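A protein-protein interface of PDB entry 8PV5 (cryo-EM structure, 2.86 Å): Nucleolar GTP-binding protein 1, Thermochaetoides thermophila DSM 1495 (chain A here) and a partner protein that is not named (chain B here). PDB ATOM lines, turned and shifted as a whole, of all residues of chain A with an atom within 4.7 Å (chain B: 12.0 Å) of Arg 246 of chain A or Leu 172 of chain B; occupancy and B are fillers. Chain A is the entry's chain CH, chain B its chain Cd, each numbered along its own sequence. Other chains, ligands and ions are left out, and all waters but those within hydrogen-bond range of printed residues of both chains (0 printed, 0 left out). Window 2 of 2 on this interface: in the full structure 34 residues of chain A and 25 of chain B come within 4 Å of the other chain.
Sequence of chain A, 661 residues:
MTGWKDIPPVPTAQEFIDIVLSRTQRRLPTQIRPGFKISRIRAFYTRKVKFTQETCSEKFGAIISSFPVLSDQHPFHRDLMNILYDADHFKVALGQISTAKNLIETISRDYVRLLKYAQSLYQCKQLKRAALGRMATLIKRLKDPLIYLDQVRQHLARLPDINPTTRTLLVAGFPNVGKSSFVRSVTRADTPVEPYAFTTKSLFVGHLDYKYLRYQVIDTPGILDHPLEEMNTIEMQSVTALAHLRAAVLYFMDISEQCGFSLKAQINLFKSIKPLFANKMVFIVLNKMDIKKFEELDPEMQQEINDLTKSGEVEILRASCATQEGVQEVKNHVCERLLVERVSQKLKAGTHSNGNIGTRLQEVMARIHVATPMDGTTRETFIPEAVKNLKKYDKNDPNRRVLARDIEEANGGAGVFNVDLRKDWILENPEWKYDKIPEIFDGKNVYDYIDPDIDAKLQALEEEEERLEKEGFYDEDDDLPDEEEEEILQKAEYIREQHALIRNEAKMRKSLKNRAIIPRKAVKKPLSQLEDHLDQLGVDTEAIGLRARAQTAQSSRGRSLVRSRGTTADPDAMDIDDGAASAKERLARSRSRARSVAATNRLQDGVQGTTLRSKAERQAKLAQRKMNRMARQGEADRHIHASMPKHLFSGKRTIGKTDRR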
ATOM      1  N   HIS A  74      25.231  21.499  16.283  1.00  0.00           N
ATOM      2  CA  HIS A  74      25.356  20.253  15.550  1.00  0.00           C
ATOM      3  C   HIS A  74      25.802  19.158  16.518  1.00  0.00           C
ATOM      4  O   HIS A  74      26.479  19.447  17.510  1.00  0.00           O
ATOM      5  CB  HIS A  74      26.363  20.422  14.412  1.00  0.00           C
ATOM      6  CG  HIS A  74      26.389  19.286  13.437  1.00  0.00           C
ATOM      7  ND1 HIS A  74      27.112  18.134  13.654  1.00  0.00           N
ATOM      8  CD2 HIS A  74      25.779  19.125  12.240  1.00  0.00           C
ATOM      9  CE1 HIS A  74      26.947  17.313  12.633  1.00  0.00           C
ATOM     10  NE2 HIS A  74      26.142  17.891  11.762  1.00  0.00           N
ATOM     11  N   PRO A  75      25.392  17.902  16.288  1.00  0.00           N
ATOM     12  CA  PRO A  75      25.814  16.814  17.191  1.00  0.00           C
ATOM     13  C   PRO A  75      27.319  16.650  17.320  1.00  0.00           C
ATOM     14  O   PRO A  75      27.802  16.294  18.404  1.00  0.00           O
ATOM     15  CB  PRO A  75      25.164  15.580  16.556  1.00  0.00           C
ATOM     16  CG  PRO A  75      23.945  16.105  15.909  1.00  0.00           C
ATOM     17  CD  PRO A  75      24.272  17.489  15.424  1.00  0.00           C
ATOM     18  N   THR A 166      30.441  20.101   5.024  1.00  0.00           N
ATOM     19  CA  THR A 166      31.246  20.435   3.855  1.00  0.00           C
ATOM     20  C   THR A 166      32.159  19.266   3.494  1.00  0.00           C
ATOM     21  O   THR A 166      32.140  18.208   4.129  1.00  0.00           O
ATOM     22  CB  THR A 166      32.058  21.710   4.098  1.00  0.00           C
ATOM     23  OG1 THR A 166      32.678  22.123   2.874  1.00  0.00           O
ATOM     24  CG2 THR A 166      33.130  21.470   5.143  1.00  0.00           C
ATOM     25  N   THR A 168      35.308  17.155   3.463  1.00  0.00           N
ATOM     26  CA  THR A 168      36.304  16.999   4.513  1.00  0.00           C
ATOM     27  C   THR A 168      37.005  15.643   4.465  1.00  0.00           C
ATOM     28  O   THR A 168      36.384  14.600   4.227  1.00  0.00           O
ATOM     29  CB  THR A 168      35.665  17.238   5.896  1.00  0.00           C
ATOM     30  OG1 THR A 168      36.629  17.017   6.934  1.00  0.00           O
ATOM     31  CG2 THR A 168      34.418  16.397   6.102  1.00  0.00           C
ATOM     32  N   HIS A 244      30.810  11.442  14.138  1.00  0.00           N
ATOM     33  CA  HIS A 244      29.791  12.452  13.889  1.00  0.00           C
ATOM     34  C   HIS A 244      29.989  13.260  12.616  1.00  0.00           C
ATOM     35  O   HIS A 244      29.040  13.914  12.173  1.00  0.00           O
ATOM     36  CB  HIS A 244      29.708  13.415  15.081  1.00  0.00           C
ATOM     37  CG  HIS A 244      29.142  12.788  16.316  1.00  0.00           C
ATOM     38  ND1 HIS A 244      29.936  12.301  17.332  1.00  0.00           N
ATOM     39  CD2 HIS A 244      27.862  12.562  16.697  1.00  0.00           C
ATOM     40  CE1 HIS A 244      29.170  11.798  18.283  1.00  0.00           C
ATOM     41  NE2 HIS A 244      27.908  11.948  17.925  1.00  0.00           N
ATOM     42  N   LEU A 245      31.175  13.238  12.016  1.00  0.00           N
ATOM     43  CA  LEU A 245      31.455  14.007  10.807  1.00  0.00           C
ATOM     44  C   LEU A 245      31.394  13.081   9.600  1.00  0.00           C
ATOM     45  O   LEU A 245      32.163  12.120   9.509  1.00  0.00           O
ATOM     46  CB  LEU A 245      32.820  14.682  10.891  1.00  0.00           C
ATOM     47  CG  LEU A 245      32.975  15.836  11.876  1.00  0.00           C
ATOM     48  CD1 LEU A 245      34.429  16.234  11.973  1.00  0.00           C
ATOM     49  CD2 LEU A 245      32.134  17.009  11.431  1.00  0.00           C
ATOM     50  N   ARG A 246      30.489  13.377   8.671  1.00  0.00           N
ATOM     51  CA  ARG A 246      30.473  12.675   7.395  1.00  0.00           C
ATOM     52  C   ARG A 246      31.654  13.147   6.557  1.00  0.00           C
ATOM     53  O   ARG A 246      31.687  14.298   6.109  1.00  0.00           O
ATOM     54  CB  ARG A 246      29.153  12.919   6.669  1.00  0.00           C
ATOM     55  CG  ARG A 246      29.004  12.134   5.377  1.00  0.00           C
ATOM     56  CD  ARG A 246      27.655  12.396   4.727  1.00  0.00           C
ATOM     57  NE  ARG A 246      26.550  11.921   5.552  1.00  0.00           N
ATOM     58  CZ  ARG A 246      25.660  12.709   6.140  1.00  0.00           C
ATOM     59  NH1 ARG A 246      25.712  14.025   6.014  1.00  0.00           N
ATOM     60  NH2 ARG A 246      24.695  12.163   6.873  1.00  0.00           N
ATOM     61  N   ALA A 247      32.622  12.262   6.346  1.00  0.00           N
ATOM     62  CA  ALA A 247      33.915  12.650   5.800  1.00  0.00           C
ATOM     63  C   ALA A 247      34.418  11.541   4.890  1.00  0.00           C
ATOM     64  O   ALA A 247      33.741  10.533   4.669  1.00  0.00           O
ATOM     65  CB  ALA A 247      34.920  12.924   6.922  1.00  0.00           C
ATOM     66  N   ASN A 279      28.176   4.635   5.859  1.00  0.00           N
ATOM     67  CA  ASN A 279      27.850   5.699   4.909  1.00  0.00           C
ATOM     68  C   ASN A 279      29.025   6.631   4.641  1.00  0.00           C
ATOM     69  O   ASN A 279      28.812   7.806   4.314  1.00  0.00           O
ATOM     70  CB  ASN A 279      26.635   6.520   5.357  1.00  0.00           C
ATOM     71  CG  ASN A 279      25.366   5.697   5.418  1.00  0.00           C
ATOM     72  OD1 ASN A 279      24.799   5.487   6.491  1.00  0.00           O
ATOM     73  ND2 ASN A 279      24.910   5.225   4.264  1.00  0.00           N
ATOM     74  N   LYS A 280      30.259   6.146   4.771  1.00  0.00           N
ATOM     75  CA  LYS A 280      31.451   6.938   4.502  1.00  0.00           C
ATOM     76  C   LYS A 280      32.414   6.110   3.666  1.00  0.00           C
ATOM     77  O   LYS A 280      32.346   4.880   3.638  1.00  0.00           O
ATOM     78  CB  LYS A 280      32.154   7.392   5.793  1.00  0.00           C
ATOM     79  CG  LYS A 280      31.269   8.119   6.790  1.00  0.00           C
ATOM     80  CD  LYS A 280      32.056   8.543   8.017  1.00  0.00           C
ATOM     81  CE  LYS A 280      31.130   9.041   9.111  1.00  0.00           C
ATOM     82  NZ  LYS A 280      31.888   9.637  10.245  1.00  0.00           N
ATOM     83  N   SER B 157      27.276   8.631  27.153  1.00  0.00           N
ATOM     84  CA  SER B 157      25.948   8.035  27.165  1.00  0.00           C
ATOM     85  C   SER B 157      25.878   6.768  26.325  1.00  0.00           C
ATOM     86  O   SER B 157      24.779   6.262  26.071  1.00  0.00           O
ATOM     87  CB  SER B 157      24.911   9.045  26.673  1.00  0.00           C
ATOM     88  OG  SER B 157      25.038   9.265  25.280  1.00  0.00           O
ATOM     89  N   PHE B 158      27.022   6.250  25.885  1.00  0.00           N
ATOM     90  CA  PHE B 158      27.069   5.078  25.026  1.00  0.00           C
ATOM     91  C   PHE B 158      28.098   4.099  25.571  1.00  0.00           C
ATOM     92  O   PHE B 158      29.059   4.480  26.242  1.00  0.00           O
ATOM     93  CB  PHE B 158      27.392   5.454  23.572  1.00  0.00           C
ATOM     94  CG  PHE B 158      28.392   6.569  23.439  1.00  0.00           C
ATOM     95  CD1 PHE B 158      29.750   6.304  23.451  1.00  0.00           C
ATOM     96  CD2 PHE B 158      27.971   7.882  23.289  1.00  0.00           C
ATOM     97  CE1 PHE B 158      30.670   7.329  23.328  1.00  0.00           C
ATOM     98  CE2 PHE B 158      28.887   8.909  23.167  1.00  0.00           C
ATOM     99  CZ  PHE B 158      30.238   8.631  23.187  1.00  0.00           C
ATOM    100  N   GLU B 163      26.478   1.198  19.526  1.00  0.00           N
ATOM    101  CA  GLU B 163      25.595   2.140  20.200  1.00  0.00           C
ATOM    102  C   GLU B 163      26.031   3.578  19.969  1.00  0.00           C
ATOM    103  O   GLU B 163      25.183   4.471  19.897  1.00  0.00           O
ATOM    104  CB  GLU B 163      25.526   1.836  21.696  1.00  0.00           C
ATOM    105  CG  GLU B 163      24.830   0.527  22.020  1.00  0.00           C
ATOM    106  CD  GLU B 163      24.803   0.239  23.504  1.00  0.00           C
ATOM    107  OE1 GLU B 163      25.387   1.032  24.269  1.00  0.00           O
ATOM    108  OE2 GLU B 163      24.200  -0.778  23.907  1.00  0.00           O
ATOM    109  N   LEU B 164      27.338   3.822  19.836  1.00  0.00           N
ATOM    110  CA  LEU B 164      27.810   5.156  19.473  1.00  0.00           C
ATOM    111  C   LEU B 164      27.343   5.549  18.076  1.00  0.00           C
ATOM    112  O   LEU B 164      26.944   6.698  17.849  1.00  0.00           O
ATOM    113  CB  LEU B 164      29.334   5.215  19.563  1.00  0.00           C
ATOM    114  CG  LEU B 164      30.022   6.492  19.073  1.00  0.00           C
ATOM    115  CD1 LEU B 164      29.489   7.726  19.781  1.00  0.00           C
ATOM    116  CD2 LEU B 164      31.518   6.376  19.259  1.00  0.00           C
ATOM    117  N   ALA B 165      27.388   4.609  17.130  1.00  0.00           N
ATOM    118  CA  ALA B 165      26.908   4.891  15.779  1.00  0.00           C
ATOM    119  C   ALA B 165      25.409   5.174  15.770  1.00  0.00           C
ATOM    120  O   ALA B 165      24.951   6.123  15.118  1.00  0.00           O
ATOM    121  CB  ALA B 165      27.241   3.725  14.850  1.00  0.00           C
ATOM    122  N   GLY B 166      24.633   4.368  16.502  1.00  0.00           N
ATOM    123  CA  GLY B 166      23.203   4.623  16.605  1.00  0.00           C
ATOM    124  C   GLY B 166      22.890   5.942  17.287  1.00  0.00           C
ATOM    125  O   GLY B 166      21.952   6.646  16.900  1.00  0.00           O
ATOM    126  N   TYR B 167      23.683   6.299  18.301  1.00  0.00           N
ATOM    127  CA  TYR B 167      23.529   7.582  18.976  1.00  0.00           C
ATOM    128  C   TYR B 167      23.821   8.740  18.034  1.00  0.00           C
ATOM    129  O   TYR B 167      23.119   9.755  18.056  1.00  0.00           O
ATOM    130  CB  TYR B 167      24.444   7.632  20.200  1.00  0.00           C
ATOM    131  CG  TYR B 167      24.660   9.012  20.774  1.00  0.00           C
ATOM    132  CD1 TYR B 167      23.656   9.655  21.486  1.00  0.00           C
ATOM    133  CD2 TYR B 167      25.877   9.667  20.620  1.00  0.00           C
ATOM    134  CE1 TYR B 167      23.853  10.915  22.018  1.00  0.00           C
ATOM    135  CE2 TYR B 167      26.082  10.927  21.147  1.00  0.00           C
ATOM    136  CZ  TYR B 167      25.068  11.545  21.845  1.00  0.00           C
ATOM    137  OH  TYR B 167      25.271  12.799  22.373  1.00  0.00           O
ATOM    138  N   SER B 168      24.850   8.601  17.193  1.00  0.00           N
ATOM    139  CA  SER B 168      25.165   9.645  16.221  1.00  0.00           C
ATOM    140  C   SER B 168      24.042   9.807  15.203  1.00  0.00           C
ATOM    141  O   SER B 168      23.659  10.934  14.859  1.00  0.00           O
ATOM    142  CB  SER B 168      26.486   9.328  15.520  1.00  0.00           C
ATOM    143  OG  SER B 168      26.418   8.087  14.842  1.00  0.00           O
ATOM    144  N   GLU B 169      23.487   8.687  14.723  1.00  0.00           N
ATOM    145  CA  GLU B 169      22.391   8.759  13.757  1.00  0.00           C
ATOM    146  C   GLU B 169      21.145   9.398  14.365  1.00  0.00           C
ATOM    147  O   GLU B 169      20.508  10.258  13.739  1.00  0.00           O
ATOM    148  CB  GLU B 169      22.066   7.368  13.207  1.00  0.00           C
ATOM    149  CG  GLU B 169      23.213   6.682  12.479  1.00  0.00           C
ATOM    150  CD  GLU B 169      23.580   7.352  11.166  1.00  0.00           C
ATOM    151  OE1 GLU B 169      24.711   7.131  10.686  1.00  0.00           O
ATOM    152  OE2 GLU B 169      22.735   8.078  10.599  1.00  0.00           O
ATOM    153  N   GLN B 170      20.788   9.010  15.593  1.00  0.00           N
ATOM    154  CA  GLN B 170      19.582   9.571  16.197  1.00  0.00           C
ATOM    155  C   GLN B 170      19.794  11.027  16.606  1.00  0.00           C
ATOM    156  O   GLN B 170      18.853  11.828  16.567  1.00  0.00           O
ATOM    157  CB  GLN B 170      19.121   8.717  17.382  1.00  0.00           C
ATOM    158  CG  GLN B 170      20.028   8.716  18.594  1.00  0.00           C
ATOM    159  CD  GLN B 170      19.545   7.767  19.674  1.00  0.00           C
ATOM    160  OE1 GLN B 170      18.499   7.134  19.537  1.00  0.00           O
ATOM    161  NE2 GLN B 170      20.308   7.663  20.756  1.00  0.00           N
ATOM    162  N   SER B 171      21.029  11.398  16.961  1.00  0.00           N
ATOM    163  CA  SER B 171      21.333  12.793  17.256  1.00  0.00           C
ATOM    164  C   SER B 171      21.223  13.653  16.006  1.00  0.00           C
ATOM    165  O   SER B 171      20.699  14.771  16.054  1.00  0.00           O
ATOM    166  CB  SER B 171      22.730  12.906  17.867  1.00  0.00           C
ATOM    167  OG  SER B 171      22.781  12.283  19.137  1.00  0.00           O
ATOM    168  N   LEU B 172      21.708  13.139  14.870  1.00  0.00           N
ATOM    169  CA  LEU B 172      21.569  13.869  13.613  1.00  0.00           C
ATOM    170  C   LEU B 172      20.105  14.002  13.206  1.00  0.00           C
ATOM    171  O   LEU B 172      19.685  15.062  12.727  1.00  0.00           O
ATOM    172  CB  LEU B 172      22.371  13.177  12.513  1.00  0.00           C
ATOM    173  CG  LEU B 172      22.546  13.979  11.222  1.00  0.00           C
ATOM    174  CD1 LEU B 172      23.236  15.303  11.508  1.00  0.00           C
ATOM    175  CD2 LEU B 172      23.323  13.177  10.194  1.00  0.00           C
ATOM    176  N   ASP B 173      19.317  12.938  13.395  1.00  0.00           N
ATOM    177  CA  ASP B 173      17.892  12.998  13.075  1.00  0.00           C
ATOM    178  C   ASP B 173      17.169  14.017  13.948  1.00  0.00           C
ATOM    179  O   ASP B 173      16.351  14.804  13.455  1.00  0.00           O
ATOM    180  CB  ASP B 173      17.262  11.614  13.229  1.00  0.00           C
ATOM    181  CG  ASP B 173      17.567  10.702  12.060  1.00  0.00           C
ATOM    182  OD1 ASP B 173      17.959  11.216  10.991  1.00  0.00           O
ATOM    183  OD2 ASP B 173      17.414   9.472  12.208  1.00  0.00           O
ATOM    184  N   SER B 174      17.473  14.029  15.250  1.00  0.00           N
ATOM    185  CA  SER B 174      16.853  14.994  16.154  1.00  0.00           C
ATOM    186  C   SER B 174      17.274  16.422  15.824  1.00  0.00           C
ATOM    187  O   SER B 174      16.457  17.347  15.896  1.00  0.00           O
ATOM    188  CB  SER B 174      17.206  14.655  17.602  1.00  0.00           C
ATOM    189  OG  SER B 174      16.724  15.649  18.487  1.00  0.00           O
ATOM    190  N   TYR B 175      18.544  16.617  15.461  1.00  0.00           N
ATOM    191  CA  TYR B 175      19.034  17.944  15.103  1.00  0.00           C
ATOM    192  C   TYR B 175      18.354  18.463  13.840  1.00  0.00           C
ATOM    193  O   TYR B 175      17.938  19.628  13.777  1.00  0.00           O
ATOM    194  CB  TYR B 175      20.553  17.889  14.934  1.00  0.00           C
ATOM    195  CG  TYR B 175      21.185  19.121  14.336  1.00  0.00           C
ATOM    196  CD1 TYR B 175      21.211  20.322  15.033  1.00  0.00           C
ATOM    197  CD2 TYR B 175      21.787  19.074  13.087  1.00  0.00           C
ATOM    198  CE1 TYR B 175      21.798  21.446  14.491  1.00  0.00           C
ATOM    199  CE2 TYR B 175      22.379  20.191  12.539  1.00  0.00           C
ATOM    200  CZ  TYR B 175      22.382  21.374  13.245  1.00  0.00           C
ATOM    201  OH  TYR B 175      22.970  22.492  12.700  1.00  0.00           O
ATOM    202  N   HIS B 176      18.202  17.596  12.833  1.00  0.00           N
ATOM    203  CA  HIS B 176      17.491  17.984  11.619  1.00  0.00           C
ATOM    204  C   HIS B 176      16.022  18.274  11.902  1.00  0.00           C
ATOM    205  O   HIS B 176      15.446  19.205  11.326  1.00  0.00           O
ATOM    206  CB  HIS B 176      17.625  16.895  10.555  1.00  0.00           C
ATOM    207  CG  HIS B 176      18.982  16.825   9.929  1.00  0.00           C
ATOM    208  ND1 HIS B 176      19.659  17.944   9.495  1.00  0.00           N
ATOM    209  CD2 HIS B 176      19.786  15.770   9.656  1.00  0.00           C
ATOM    210  CE1 HIS B 176      20.824  17.582   8.987  1.00  0.00           C
ATOM    211  NE2 HIS B 176      20.925  16.268   9.072  1.00  0.00           N
ATOM    212  N   ALA B 177      15.402  17.488  12.786  1.00  0.00           N
ATOM    213  CA  ALA B 177      14.005  17.720  13.142  1.00  0.00           C
ATOM    214  C   ALA B 177      13.827  19.061  13.846  1.00  0.00           C
ATOM    215  O   ALA B 177      12.861  19.788  13.584  1.00  0.00           O
ATOM    216  CB  ALA B 177      13.491  16.578  14.019  1.00  0.00           C
ATOM    217  N   ARG B 178      14.756  19.410  14.740  1.00  0.00           N
ATOM    218  CA  ARG B 178      14.658  20.694  15.428  1.00  0.00           C
ATOM    219  C   ARG B 178      14.907  21.860  14.478  1.00  0.00           C
ATOM    220  O   ARG B 178      14.259  22.907  14.597  1.00  0.00           O
ATOM    221  CB  ARG B 178      15.623  20.750  16.612  1.00  0.00           C
ATOM    222  CG  ARG B 178      15.301  19.764  17.721  1.00  0.00           C
ATOM    223  CD  ARG B 178      16.305  19.860  18.856  1.00  0.00           C
ATOM    224  NE  ARG B 178      16.215  21.140  19.548  1.00  0.00           N
ATOM    225  CZ  ARG B 178      17.132  22.096  19.482  1.00  0.00           C
ATOM    226  NH1 ARG B 178      18.230  21.952  18.759  1.00  0.00           N
ATOM    227  NH2 ARG B 178      16.940  23.226  20.157  1.00  0.00           N
ATOM    228  N   LEU B 179      15.834  21.700  13.525  1.00  0.00           N
ATOM    229  CA  LEU B 179      16.028  22.744  12.517  1.00  0.00           C
ATOM    230  C   LEU B 179      14.784  22.922  11.656  1.00  0.00           C
ATOM    231  O   LEU B 179      14.403  24.052  11.329  1.00  0.00           O
ATOM    232  CB  LEU B 179      17.235  22.437  11.632  1.00  0.00           C
ATOM    233  CG  LEU B 179      18.637  22.436  12.229  1.00  0.00           C
ATOM    234  CD1 LEU B 179      19.608  21.969  11.166  1.00  0.00           C
ATOM    235  CD2 LEU B 179      19.008  23.818  12.736  1.00  0.00           C
ATOM    236  N   GLU B 180      14.143  21.815  11.270  1.00  0.00           N
ATOM    237  CA  GLU B 180      12.924  21.906  10.473  1.00  0.00           C
ATOM    238  C   GLU B 180      11.793  22.560  11.258  1.00  0.00           C
ATOM    239  O   GLU B 180      11.027  23.360  10.707  1.00  0.00           O
ATOM    240  CB  GLU B 180      12.508  20.518   9.985  1.00  0.00           C
ATOM    241  CG  GLU B 180      13.360  19.978   8.844  1.00  0.00           C
ATOM    242  CD  GLU B 180      13.056  20.641   7.511  1.00  0.00           C
ATOM    243  OE1 GLU B 180      11.989  21.277   7.383  1.00  0.00           O
ATOM    244  OE2 GLU B 180      13.891  20.526   6.589  1.00  0.00           O
ATOM    245  N   GLU B 181      11.681  22.240  12.550  1.00  0.00           N
ATOM    246  CA  GLU B 181      10.650  22.849  13.386  1.00  0.00           C
ATOM    247  C   GLU B 181      10.898  24.345  13.559  1.00  0.00           C
ATOM    248  O   GLU B 181       9.958  25.147  13.539  1.00  0.00           O
ATOM    249  CB  GLU B 181      10.595  22.133  14.741  1.00  0.00           C
ATOM    250  CG  GLU B 181       9.412  22.495  15.645  1.00  0.00           C
ATOM    251  CD  GLU B 181       9.636  23.752  16.467  1.00  0.00           C
ATOM    252  OE1 GLU B 181      10.805  24.057  16.783  1.00  0.00           O
ATOM    253  OE2 GLU B 181       8.642  24.435  16.793  1.00  0.00           O
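Printed residues of chain A that touch a printed residue of chain B: His 74, Pro 75, His 244 and Arg 246. Hydrophobic or aromatic side chains of chain A within 4 Å of the printed part of chain B: His 74, Pro 75 and His 244. Printed residues of chain B that touch a printed residue of chain A: Tyr 167, Ser 168, Ser 171, Leu 172 and Tyr 175. Hydrophobic or aromatic side chains of chain B within 4 Å of the printed part of chain A: Tyr 167, Leu 172 and Tyr 175.
The backbone carbonyl oxygen of Leu 164 of chain B sits at hydrogen-bond distance from the side-chain hydroxyl of Ser 168 of chain B. The side-chain hydroxyl (OG) of Ser 168 of chain B sits at hydrogen-bond distance from the backbone carbonyl oxygen (O) of Ala 165 of chain B (2.5 Å). O of Tyr 167 of chain B lies within hydrogen-bond range of OG of Ser 171 of chain B (2.8 Å).
No residue of chain B comes within 4 Å of Thr 168 of chain A. No residue of chain B comes within 4 Å of Leu 245 of chain A. No residue of chain B comes within 4 Å of Ala 247 of chain A. Of the printed residues of chain A, Tyr 167 of chain B touches His 244. Of the printed residues of chain A, Ser 168 of chain B touches His 244. Gln 170 of chain B touches none of the printed residues of chain A. Of chain A, only His 74 (3.9 Å), Pro 75 (3.9 Å) and Arg 246 (3.7 Å) come within 4 Å of Leu 172 of chain B. His 176 of chain B touches none of the printed residues of chain A. The nearest printed residue of chain A that does not touch Leu 172 of chain B is His 244 of chain A (6.0 Å). The nearest printed residue of chain B that does not touch His 244 of chain A is Leu 164 of chain B (4.4 Å).
Among the printed residues, merely in contact across the chains: Pro 75 of chain A with Ser 171 of chain B, His 74 of chain A with Tyr 175 of chain B, Pro 75 of chain A with Tyr 175 of chain B, His 244 of chain A with Ser 168 of chain B, Arg 246 of chain A with Leu 172 of chain B, His 244 of chain A with Tyr 167 of chain B, Pro 75 of chain A with Leu 172 of chain B and His 74 of chain A with Leu 172 of chain B.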
